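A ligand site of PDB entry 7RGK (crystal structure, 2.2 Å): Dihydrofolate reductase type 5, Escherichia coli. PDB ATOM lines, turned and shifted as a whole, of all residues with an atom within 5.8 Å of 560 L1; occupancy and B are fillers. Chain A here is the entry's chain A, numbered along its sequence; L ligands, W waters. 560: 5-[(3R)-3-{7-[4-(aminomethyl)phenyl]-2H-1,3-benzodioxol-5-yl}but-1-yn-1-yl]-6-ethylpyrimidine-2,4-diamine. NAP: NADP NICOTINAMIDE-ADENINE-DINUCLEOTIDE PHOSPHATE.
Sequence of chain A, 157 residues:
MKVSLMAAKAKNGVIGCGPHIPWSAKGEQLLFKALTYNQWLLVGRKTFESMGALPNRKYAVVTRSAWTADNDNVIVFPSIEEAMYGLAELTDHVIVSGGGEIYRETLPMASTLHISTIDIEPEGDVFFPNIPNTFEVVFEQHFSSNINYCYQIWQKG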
ATOM      1  N   MET A   6      33.611 -17.376 -22.810  1.00  0.00           N
ATOM      2  CA  MET A   6      33.676 -16.897 -21.436  1.00  0.00           C
ATOM      3  C   MET A   6      33.470 -18.037 -20.456  1.00  0.00           C
ATOM      4  O   MET A   6      32.415 -18.680 -20.472  1.00  0.00           O
ATOM      5  CB  MET A   6      32.660 -15.793 -21.183  1.00  0.00           C
ATOM      6  CG  MET A   6      32.896 -15.182 -19.829  1.00  0.00           C
ATOM      7  SD  MET A   6      32.424 -13.449 -19.739  1.00  0.00           S
ATOM      8  CE  MET A   6      33.198 -13.078 -18.158  1.00  0.00           C
ATOM      9  N   ALA A   7      34.444 -18.260 -19.566  1.00  0.00           N
ATOM     10  CA  ALA A   7      34.322 -19.353 -18.617  1.00  0.00           C
ATOM     11  C   ALA A   7      34.984 -18.987 -17.296  1.00  0.00           C
ATOM     12  O   ALA A   7      35.842 -18.113 -17.218  1.00  0.00           O
ATOM     13  CB  ALA A   7      34.933 -20.638 -19.190  1.00  0.00           C
ATOM     14  N   ALA A   8      34.548 -19.681 -16.243  1.00  0.00           N
ATOM     15  CA  ALA A   8      35.183 -19.652 -14.937  1.00  0.00           C
ATOM     16  C   ALA A   8      35.627 -21.068 -14.606  1.00  0.00           C
ATOM     17  O   ALA A   8      34.844 -22.004 -14.785  1.00  0.00           O
ATOM     18  CB  ALA A   8      34.230 -19.153 -13.839  1.00  0.00           C
ATOM     19  N   PRO A  19      25.352 -31.177 -12.312  1.00  0.00           N
ATOM     20  CA  PRO A  19      24.802 -29.986 -12.974  1.00  0.00           C
ATOM     21  C   PRO A  19      25.157 -28.661 -12.307  1.00  0.00           C
ATOM     22  O   PRO A  19      24.644 -27.624 -12.737  1.00  0.00           O
ATOM     23  CB  PRO A  19      23.289 -30.240 -12.890  1.00  0.00           C
ATOM     24  CG  PRO A  19      23.129 -30.942 -11.604  1.00  0.00           C
ATOM     25  CD  PRO A  19      24.360 -31.817 -11.426  1.00  0.00           C
ATOM     26  N   HIS A  20      26.012 -28.658 -11.281  1.00  0.00           N
ATOM     27  CA  HIS A  20      26.320 -27.471 -10.496  1.00  0.00           C
ATOM     28  C   HIS A  20      27.733 -26.975 -10.798  1.00  0.00           C
ATOM     29  O   HIS A  20      28.602 -27.741 -11.215  1.00  0.00           O
ATOM     30  CB  HIS A  20      26.195 -27.744  -8.998  1.00  0.00           C
ATOM     31  CG  HIS A  20      24.848 -28.247  -8.572  1.00  0.00           C
ATOM     32  ND1 HIS A  20      23.724 -27.443  -8.561  1.00  0.00           N
ATOM     33  CD2 HIS A  20      24.442 -29.473  -8.146  1.00  0.00           C
ATOM     34  CE1 HIS A  20      22.689 -28.150  -8.141  1.00  0.00           C
ATOM     35  NE2 HIS A  20      23.093 -29.381  -7.888  1.00  0.00           N
ATOM     36  N   ILE A  21      27.956 -25.690 -10.544  1.00  0.00           N
ATOM     37  CA  ILE A  21      29.292 -25.118 -10.510  1.00  0.00           C
ATOM     38  C   ILE A  21      29.761 -25.114  -9.060  1.00  0.00           C
ATOM     39  O   ILE A  21      29.124 -24.449  -8.228  1.00  0.00           O
ATOM     40  CB  ILE A  21      29.332 -23.710 -11.112  1.00  0.00           C
ATOM     41  CG1 ILE A  21      29.059 -23.769 -12.612  1.00  0.00           C
ATOM     42  CG2 ILE A  21      30.691 -23.055 -10.885  1.00  0.00           C
ATOM     43  CD1 ILE A  21      28.369 -22.531 -13.148  1.00  0.00           C
ATOM     44  N   GLU A  28      32.573 -12.527  -8.937  1.00  0.00           N
ATOM     45  CA  GLU A  28      32.935 -13.087 -10.240  1.00  0.00           C
ATOM     46  C   GLU A  28      31.791 -12.991 -11.234  1.00  0.00           C
ATOM     47  O   GLU A  28      32.008 -12.693 -12.417  1.00  0.00           O
ATOM     48  CB  GLU A  28      33.374 -14.554 -10.109  1.00  0.00           C
ATOM     49  CG  GLU A  28      34.271 -15.013 -11.275  1.00  0.00           C
ATOM     50  CD  GLU A  28      33.506 -15.285 -12.570  1.00  0.00           C
ATOM     51  OE1 GLU A  28      32.445 -15.974 -12.505  1.00  0.00           O
ATOM     52  OE2 GLU A  28      33.940 -14.813 -13.653  1.00  0.00           O
ATOM     53  N   GLN A  29      30.569 -13.241 -10.765  1.00  0.00           N
ATOM     54  CA  GLN A  29      29.380 -13.194 -11.617  1.00  0.00           C
ATOM     55  C   GLN A  29      29.235 -11.829 -12.308  1.00  0.00           C
ATOM     56  O   GLN A  29      28.697 -11.755 -13.419  1.00  0.00           O
ATOM     57  CB  GLN A  29      28.166 -13.528 -10.748  1.00  0.00           C
ATOM     58  CG  GLN A  29      26.786 -13.440 -11.365  1.00  0.00           C
ATOM     59  CD  GLN A  29      25.719 -13.916 -10.379  1.00  0.00           C
ATOM     60  OE1 GLN A  29      24.711 -13.241 -10.169  1.00  0.00           O
ATOM     61  NE2 GLN A  29      25.932 -15.084  -9.781  1.00  0.00           N
ATOM     62  N   LEU A  31      31.534  -9.931 -13.717  1.00  0.00           N
ATOM     63  CA  LEU A  31      32.243  -9.953 -14.990  1.00  0.00           C
ATOM     64  C   LEU A  31      31.404 -10.612 -16.059  1.00  0.00           C
ATOM     65  O   LEU A  31      31.243 -10.082 -17.160  1.00  0.00           O
ATOM     66  CB  LEU A  31      33.572 -10.688 -14.848  1.00  0.00           C
ATOM     67  CG  LEU A  31      34.585 -10.025 -13.929  1.00  0.00           C
ATOM     68  CD1 LEU A  31      35.672 -11.020 -13.583  1.00  0.00           C
ATOM     69  CD2 LEU A  31      35.152  -8.784 -14.601  1.00  0.00           C
ATOM     70  N   PHE A  32      30.831 -11.779 -15.738  1.00  0.00           N
ATOM     71  CA  PHE A  32      30.042 -12.505 -16.716  1.00  0.00           C
ATOM     72  C   PHE A  32      28.817 -11.697 -17.131  1.00  0.00           C
ATOM     73  O   PHE A  32      28.518 -11.564 -18.319  1.00  0.00           O
ATOM     74  CB  PHE A  32      29.643 -13.857 -16.147  1.00  0.00           C
ATOM     75  CG  PHE A  32      28.684 -14.615 -17.015  1.00  0.00           C
ATOM     76  CD1 PHE A  32      29.129 -15.300 -18.124  1.00  0.00           C
ATOM     77  CD2 PHE A  32      27.329 -14.638 -16.711  1.00  0.00           C
ATOM     78  CE1 PHE A  32      28.234 -16.017 -18.931  1.00  0.00           C
ATOM     79  CE2 PHE A  32      26.441 -15.339 -17.494  1.00  0.00           C
ATOM     80  CZ  PHE A  32      26.895 -16.026 -18.620  1.00  0.00           C
ATOM     81  N   LYS A  33      28.069 -11.162 -16.147  1.00  0.00           N
ATOM     82  CA  LYS A  33      26.910 -10.337 -16.473  1.00  0.00           C
ATOM     83  C   LYS A  33      27.305  -9.106 -17.278  1.00  0.00           C
ATOM     84  O   LYS A  33      26.637  -8.755 -18.253  1.00  0.00           O
ATOM     85  CB  LYS A  33      26.165  -9.947 -15.187  1.00  0.00           C
ATOM     86  CG  LYS A  33      25.398 -11.116 -14.535  1.00  0.00           C
ATOM     87  CD  LYS A  33      24.022 -10.686 -14.006  1.00  0.00           C
ATOM     88  CE  LYS A  33      23.322 -11.802 -13.237  1.00  0.00           C
ATOM     89  NZ  LYS A  33      21.855 -11.895 -13.513  1.00  0.00           N
ATOM     90  N   VAL A  43      25.121 -21.679 -25.914  1.00  0.00           N
ATOM     91  CA  VAL A  43      25.227 -22.603 -24.790  1.00  0.00           C
ATOM     92  C   VAL A  43      24.688 -23.968 -25.173  1.00  0.00           C
ATOM     93  O   VAL A  43      23.825 -24.098 -26.051  1.00  0.00           O
ATOM     94  CB  VAL A  43      24.480 -22.109 -23.552  1.00  0.00           C
ATOM     95  CG1 VAL A  43      25.238 -20.991 -22.912  1.00  0.00           C
ATOM     96  CG2 VAL A  43      23.080 -21.680 -23.939  1.00  0.00           C
ATOM     97  N   THR A  47      23.285 -26.864 -20.102  1.00  0.00           N
ATOM     98  CA  THR A  47      23.554 -25.632 -19.376  1.00  0.00           C
ATOM     99  C   THR A  47      22.385 -24.674 -19.488  1.00  0.00           C
ATOM    100  O   THR A  47      21.991 -24.048 -18.504  1.00  0.00           O
ATOM    101  CB  THR A  47      24.836 -24.994 -19.899  1.00  0.00           C
ATOM    102  OG1 THR A  47      25.952 -25.784 -19.474  1.00  0.00           O
ATOM    103  CG2 THR A  47      25.009 -23.568 -19.372  1.00  0.00           C
ATOM    104  N   SER A  50      19.784 -25.547 -17.009  1.00  0.00           N
ATOM    105  CA  SER A  50      20.135 -25.215 -15.640  1.00  0.00           C
ATOM    106  C   SER A  50      19.935 -23.730 -15.334  1.00  0.00           C
ATOM    107  O   SER A  50      19.403 -23.378 -14.284  1.00  0.00           O
ATOM    108  CB  SER A  50      21.576 -25.626 -15.346  1.00  0.00           C
ATOM    109  OG  SER A  50      21.731 -27.021 -15.483  1.00  0.00           O
ATOM    110  N   MET A  51      20.339 -22.848 -16.247  1.00  0.00           N
ATOM    111  CA  MET A  51      20.251 -21.429 -15.932  1.00  0.00           C
ATOM    112  C   MET A  51      18.977 -20.773 -16.455  1.00  0.00           C
ATOM    113  O   MET A  51      18.488 -19.821 -15.833  1.00  0.00           O
ATOM    114  CB  MET A  51      21.470 -20.688 -16.467  1.00  0.00           C
ATOM    115  CG  MET A  51      21.621 -20.808 -17.946  1.00  0.00           C
ATOM    116  SD  MET A  51      22.195 -19.303 -18.739  1.00  0.00           S
ATOM    117  CE  MET A  51      22.001 -19.860 -20.418  1.00  0.00           C
ATOM    118  N   LEU A  54      17.956 -15.925 -18.835  1.00  0.00           N
ATOM    119  CA  LEU A  54      18.011 -14.789 -17.925  1.00  0.00           C
ATOM    120  C   LEU A  54      17.958 -13.485 -18.730  1.00  0.00           C
ATOM    121  O   LEU A  54      18.349 -13.447 -19.892  1.00  0.00           O
ATOM    122  CB  LEU A  54      19.241 -14.871 -17.024  1.00  0.00           C
ATOM    123  CG  LEU A  54      20.692 -14.562 -17.406  1.00  0.00           C
ATOM    124  CD1 LEU A  54      20.950 -13.056 -17.310  1.00  0.00           C
ATOM    125  CD2 LEU A  54      21.676 -15.328 -16.510  1.00  0.00           C
ATOM    126  N   VAL A  96      30.461 -17.752 -26.331  1.00  0.00           N
ATOM    127  CA  VAL A  96      30.266 -19.141 -25.935  1.00  0.00           C
ATOM    128  C   VAL A  96      30.319 -19.191 -24.420  1.00  0.00           C
ATOM    129  O   VAL A  96      31.319 -18.808 -23.810  1.00  0.00           O
ATOM    130  CB  VAL A  96      31.332 -20.053 -26.550  1.00  0.00           C
ATOM    131  CG1 VAL A  96      31.259 -21.447 -25.955  1.00  0.00           C
ATOM    132  CG2 VAL A  96      31.197 -20.095 -28.061  1.00  0.00           C
ATOM    133  N   SER A  97      29.238 -19.670 -23.804  1.00  0.00           N
ATOM    134  CA  SER A  97      29.094 -19.537 -22.368  1.00  0.00           C
ATOM    135  C   SER A  97      28.952 -20.881 -21.680  1.00  0.00           C
ATOM    136  O   SER A  97      28.751 -20.923 -20.465  1.00  0.00           O
ATOM    137  CB  SER A  97      27.901 -18.659 -22.040  1.00  0.00           C
ATOM    138  OG  SER A  97      28.281 -17.317 -22.279  1.00  0.00           O
ATOM    139  N   GLY A  98      29.010 -21.968 -22.426  1.00  0.00           N
ATOM    140  CA  GLY A  98      29.373 -23.131 -21.694  1.00  0.00           C
ATOM    141  C   GLY A  98      28.483 -24.296 -21.966  1.00  0.00           C
ATOM    142  O   GLY A  98      27.698 -24.307 -22.921  1.00  0.00           O
ATOM    143  N   TYR A 103      32.376 -26.037 -24.724  1.00  0.00           N
ATOM    144  CA  TYR A 103      33.704 -25.436 -24.641  1.00  0.00           C
ATOM    145  C   TYR A 103      34.724 -26.205 -25.489  1.00  0.00           C
ATOM    146  O   TYR A 103      35.499 -25.609 -26.233  1.00  0.00           O
ATOM    147  CB  TYR A 103      34.172 -25.390 -23.186  1.00  0.00           C
ATOM    148  CG  TYR A 103      33.535 -24.316 -22.316  1.00  0.00           C
ATOM    149  CD1 TYR A 103      33.193 -23.075 -22.821  1.00  0.00           C
ATOM    150  CD2 TYR A 103      33.331 -24.556 -20.953  1.00  0.00           C
ATOM    151  CE1 TYR A 103      32.639 -22.090 -21.987  1.00  0.00           C
ATOM    152  CE2 TYR A 103      32.785 -23.591 -20.125  1.00  0.00           C
ATOM    153  CZ  TYR A 103      32.431 -22.365 -20.645  1.00  0.00           C
ATOM    154  OH  TYR A 103      31.889 -21.425 -19.789  1.00  0.00           O
ATOM    155  N   HIS A 114      37.603 -15.100 -22.314  1.00  0.00           N
ATOM    156  CA  HIS A 114      37.443 -14.462 -21.019  1.00  0.00           C
ATOM    157  C   HIS A 114      37.465 -15.543 -19.953  1.00  0.00           C
ATOM    158  O   HIS A 114      36.536 -16.340 -19.851  1.00  0.00           O
ATOM    159  CB  HIS A 114      36.141 -13.673 -20.962  1.00  0.00           C
ATOM    160  CG  HIS A 114      36.115 -12.519 -21.916  1.00  0.00           C
ATOM    161  ND1 HIS A 114      36.448 -11.235 -21.538  1.00  0.00           N
ATOM    162  CD2 HIS A 114      35.838 -12.460 -23.230  1.00  0.00           C
ATOM    163  CE1 HIS A 114      36.350 -10.426 -22.574  1.00  0.00           C
ATOM    164  NE2 HIS A 114      35.975 -11.148 -23.612  1.00  0.00           N
ATOM    165  N   ILE A 115      38.540 -15.588 -19.170  1.00  0.00           N
ATOM    166  CA  ILE A 115      38.792 -16.722 -18.273  1.00  0.00           C
ATOM    167  C   ILE A 115      38.936 -16.215 -16.862  1.00  0.00           C
ATOM    168  O   ILE A 115      39.882 -15.467 -16.553  1.00  0.00           O
ATOM    169  CB  ILE A 115      40.047 -17.505 -18.683  1.00  0.00           C
ATOM    170  CG1 ILE A 115      39.980 -17.912 -20.157  1.00  0.00           C
ATOM    171  CG2 ILE A 115      40.250 -18.696 -17.724  1.00  0.00           C
ATOM    172  CD1 ILE A 115      38.839 -18.790 -20.470  1.00  0.00           C
ATOM    173  N   SER A 116      38.036 -16.638 -15.991  1.00  0.00           N
ATOM    174  CA  SER A 116      38.178 -16.387 -14.571  1.00  0.00           C
ATOM    175  C   SER A 116      38.736 -17.636 -13.897  1.00  0.00           C
ATOM    176  O   SER A 116      38.158 -18.721 -14.031  1.00  0.00           O
ATOM    177  CB  SER A 116      36.835 -15.996 -13.952  1.00  0.00           C
ATOM    178  OG  SER A 116      36.451 -14.707 -14.394  1.00  0.00           O
HETATM  179  C4  560 L   1      30.368 -17.635 -15.062  1.00  0.00           C
HETATM  180  C5  560 L   1      29.993 -18.271 -16.235  1.00  0.00           C
HETATM  181  C6  560 L   1      30.831 -18.184 -17.356  1.00  0.00           C
HETATM  182  N1  560 L   1      31.984 -17.491 -17.261  1.00  0.00           N
HETATM  183  N3  560 L   1      31.528 -16.962 -15.018  1.00  0.00           N
HETATM  184  C2  560 L   1      32.326 -16.883 -16.101  1.00  0.00           C
HETATM  185  CAG 560 L   1      28.802 -18.945 -16.261  1.00  0.00           C
HETATM  186  CAH 560 L   1      27.724 -19.549 -16.272  1.00  0.00           C
HETATM  187  CAI 560 L   1      26.458 -20.239 -16.277  1.00  0.00           C
HETATM  188  CAJ 560 L   1      25.917 -20.209 -17.711  1.00  0.00           C
HETATM  189  CAK 560 L   1      25.525 -19.611 -15.422  1.00  0.00           C
HETATM  190  CAL 560 L   1      24.663 -20.355 -14.637  1.00  0.00           C
HETATM  191  CAM 560 L   1      23.747 -19.755 -13.781  1.00  0.00           C
HETATM  192  CAN 560 L   1      22.903 -20.615 -13.073  1.00  0.00           C
HETATM  193  CAO 560 L   1      22.892 -21.973 -13.424  1.00  0.00           C
HETATM  194  CAP 560 L   1      22.038 -22.863 -12.752  1.00  0.00           C
HETATM  195  CAQ 560 L   1      21.180 -22.440 -11.741  1.00  0.00           C
HETATM  196  CAR 560 L   1      20.340 -23.365 -11.103  1.00  0.00           C
HETATM  197  CAT 560 L   1      21.179 -21.087 -11.408  1.00  0.00           C
HETATM  198  CAU 560 L   1      22.028 -20.197 -12.071  1.00  0.00           C
HETATM  199  CAV 560 L   1      23.646 -18.398 -13.714  1.00  0.00           C
HETATM  200  CAX 560 L   1      23.310 -16.247 -13.122  1.00  0.00           C
HETATM  201  CAZ 560 L   1      24.471 -17.643 -14.474  1.00  0.00           C
HETATM  202  CBA 560 L   1      25.379 -18.218 -15.303  1.00  0.00           C
HETATM  203  CBC 560 L   1      29.522 -17.725 -13.946  1.00  0.00           C
HETATM  204  CBD 560 L   1      29.437 -16.406 -13.210  1.00  0.00           C
HETATM  205  NAA 560 L   1      33.465 -16.218 -16.033  1.00  0.00           N
HETATM  206  NAE 560 L   1      30.464 -18.809 -18.481  1.00  0.00           N
HETATM  207  NAS 560 L   1      20.711 -23.578  -9.697  1.00  0.00           N
HETATM  208  OAW 560 L   1      22.808 -17.595 -12.979  1.00  0.00           O
HETATM  209  OAY 560 L   1      24.231 -16.314 -14.248  1.00  0.00           O
HETATM  210  PA  NAP L   2      26.496 -28.742 -22.038  1.00  0.00           P
HETATM  211  O1A NAP L   2      27.672 -28.490 -22.881  1.00  0.00           O
HETATM  212  O2A NAP L   2      25.901 -27.536 -21.412  1.00  0.00           O
HETATM  213  O5B NAP L   2      25.401 -29.432 -22.984  1.00  0.00           O
HETATM  214  C5B NAP L   2      25.724 -30.576 -23.734  1.00  0.00           C
HETATM  215  C4B NAP L   2      24.511 -30.787 -24.622  1.00  0.00           C
HETATM  216  O4B NAP L   2      24.469 -29.790 -25.632  1.00  0.00           O
HETATM  217  C3B NAP L   2      24.541 -32.128 -25.328  1.00  0.00           C
HETATM  218  O3B NAP L   2      24.059 -33.135 -24.472  1.00  0.00           O
HETATM  219  C2B NAP L   2      23.655 -31.822 -26.533  1.00  0.00           C
HETATM  220  O2B NAP L   2      22.274 -31.689 -26.251  1.00  0.00           O
HETATM  221  C1B NAP L   2      24.044 -30.388 -26.836  1.00  0.00           C
HETATM  222  N9A NAP L   2      25.125 -30.321 -27.817  1.00  0.00           N
HETATM  223  C8A NAP L   2      26.455 -30.249 -27.552  1.00  0.00           C
HETATM  224  N7A NAP L   2      27.129 -30.194 -28.719  1.00  0.00           N
HETATM  225  C5A NAP L   2      26.252 -30.233 -29.751  1.00  0.00           C
HETATM  226  C6A NAP L   2      26.416 -30.209 -31.140  1.00  0.00           C
HETATM  227  N6A NAP L   2      27.618 -30.119 -31.723  1.00  0.00           N
HETATM  228  N1A NAP L   2      25.285 -30.245 -31.929  1.00  0.00           N
HETATM  229  C2A NAP L   2      24.032 -30.321 -31.340  1.00  0.00           C
HETATM  230  N3A NAP L   2      23.878 -30.357 -29.967  1.00  0.00           N
HETATM  231  C4A NAP L   2      24.977 -30.316 -29.183  1.00  0.00           C
HETATM  232  O3  NAP L   2      26.764 -29.934 -20.978  1.00  0.00           O
HETATM  233  PN  NAP L   2      27.985 -30.451 -20.082  1.00  0.00           P
HETATM  234  O1N NAP L   2      27.457 -31.557 -19.226  1.00  0.00           O
HETATM  235  O2N NAP L   2      29.143 -30.645 -20.979  1.00  0.00           O
HETATM  236  O5D NAP L   2      28.295 -29.198 -19.123  1.00  0.00           O
HETATM  237  C5D NAP L   2      27.473 -28.926 -18.019  1.00  0.00           C
HETATM  238  C4D NAP L   2      28.375 -28.618 -16.839  1.00  0.00           C
HETATM  239  O4D NAP L   2      29.189 -27.491 -17.121  1.00  0.00           O
HETATM  240  C3D NAP L   2      27.568 -28.284 -15.587  1.00  0.00           C
HETATM  241  O3D NAP L   2      28.250 -28.822 -14.479  1.00  0.00           O
HETATM  242  C2D NAP L   2      27.665 -26.782 -15.505  1.00  0.00           C
HETATM  243  O2D NAP L   2      27.591 -26.380 -14.159  1.00  0.00           O
HETATM  244  C1D NAP L   2      29.047 -26.524 -16.097  1.00  0.00           C
HETATM  245  N1N NAP L   2      29.235 -25.133 -16.576  1.00  0.00           N
HETATM  246  C2N NAP L   2      30.346 -24.456 -16.173  1.00  0.00           C
HETATM  247  C3N NAP L   2      30.564 -23.144 -16.604  1.00  0.00           C
HETATM  248  C7N NAP L   2      31.799 -22.443 -16.164  1.00  0.00           C
HETATM  249  O7N NAP L   2      32.332 -22.769 -14.922  1.00  0.00           O
HETATM  250  N7N NAP L   2      32.350 -21.535 -16.948  1.00  0.00           N
HETATM  251  C4N NAP L   2      29.662 -22.509 -17.442  1.00  0.00           C
HETATM  252  C5N NAP L   2      28.537 -23.219 -17.847  1.00  0.00           C
HETATM  253  C6N NAP L   2      28.337 -24.528 -17.408  1.00  0.00           C
HETATM  254  P2B NAP L   2      21.172 -32.874 -26.166  1.00  0.00           P
HETATM  255  O1X NAP L   2      21.264 -33.645 -27.466  1.00  0.00           O
HETATM  256  O2X NAP L   2      21.437 -33.691 -24.929  1.00  0.00           O
HETATM  257  O3X NAP L   2      19.807 -32.253 -26.085  1.00  0.00           O
HETATM  258  O   HOH W   1      35.710 -14.980 -17.362  1.00  0.00           O
HETATM  259  O   HOH W   2      25.036 -24.164 -13.819  1.00  0.00           O
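Water W1 lies within hydrogen-bond range of a nitrogen (NAA) of 560 L1 (2.9 Å), the backbone carbonyl oxygen of His 114 (3.0 Å), the side-chain hydroxyl of Ser 116 (3.1 Å), the backbone carbonyl oxygen of Ala 7 (3.1 Å) and the backbone NH of Ile 115 (3.4 Å).
A nitrogen (NAA) of 560 L1 sits at hydrogen-bond distance from the backbone carbonyl oxygen (O) of Ala 7, at 3.3 Å. A nitrogen (NAE) of 560 L1 lies within hydrogen-bond range of the backbone carbonyl oxygen (O) of Ser 97 (3.4 Å). The side-chain hydroxyl (OG1) of Thr 47 lies within hydrogen-bond range of an oxygen (O2A) of NAP L2 (2.6 Å). An oxygen (O2D) of NAP L2 lies within hydrogen-bond range of the backbone carbonyl oxygen (O) of His 20 (3.4 Å). NAE of 560 L1 lies within hydrogen-bond range of OH of Tyr 103 (3.3 Å). The backbone carbonyl oxygen (O) of Met 6 sits at hydrogen-bond distance from a nitrogen (NAE) of 560 L1, at 2.8 Å. The side-chain hydroxyl (OH) of Tyr 103 is in hydrogen-bond range of a nitrogen (N7N) of NAP L2 (2.9 Å). The side-chain carboxylate (OE2) of Glu 28 is in hydrogen-bond range of a nitrogen (NAA) of 560 L1, 2.8 Å away. N of Thr 47 is in hydrogen-bond range of O2A of NAP L2, at 3.0 Å. O of Ala 8 lies within hydrogen-bond range of N7N of NAP L2 (3.3 Å). N of Ala 7 sits close to N1 of 560 L1 (3.5 Å).
N of Ala 8 touches N1 of 560 L1, at 3.5 Å. Gln 29 touches 560 L1. Phe 32 touches 560 L1. Thr 47 touches 560 L1. Ser 50 touches 560 L1. Met 51 touches 560 L1 (CB to CAO, 3.6 Å). CD2 of Leu 54 touches OAY of 560 L1, 3.6 Å away. OG of Ser 116 touches NAA of 560 L1 (3.7 Å). Hydrophobic or aromatic side chains within 4 Å of 560 L1: Met 6, Ala 8, Phe 32, Met 51 and Leu 54. Within 4 Å of 560 L1: Met 6, Ala 7, Ala 8, Glu 28, Gln 29, Phe 32, Thr 47, Ser 50, Met 51, Leu 54, Ser 97, Tyr 103 and Ser 116.
OE2 of Glu 28 is in hydrogen-bond range of OG of Ser 116, at 2.6 Å. The backbone carbonyl oxygen of Ala 7 lies within hydrogen-bond range of the backbone NH of Ser 116 (2.9 Å). OH of Tyr 103 lies within hydrogen-bond range of O of Ser 97 (3.2 Å). The backbone carbonyl oxygen (O) of Met 6 sits at hydrogen-bond distance from the side-chain hydroxyl (OH) of Tyr 103, 2.9 Å away. N of Ala 7 lies within hydrogen-bond range of O of His 114. N of Met 6 sits at hydrogen-bond distance from O of Val 96 (2.9 Å).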
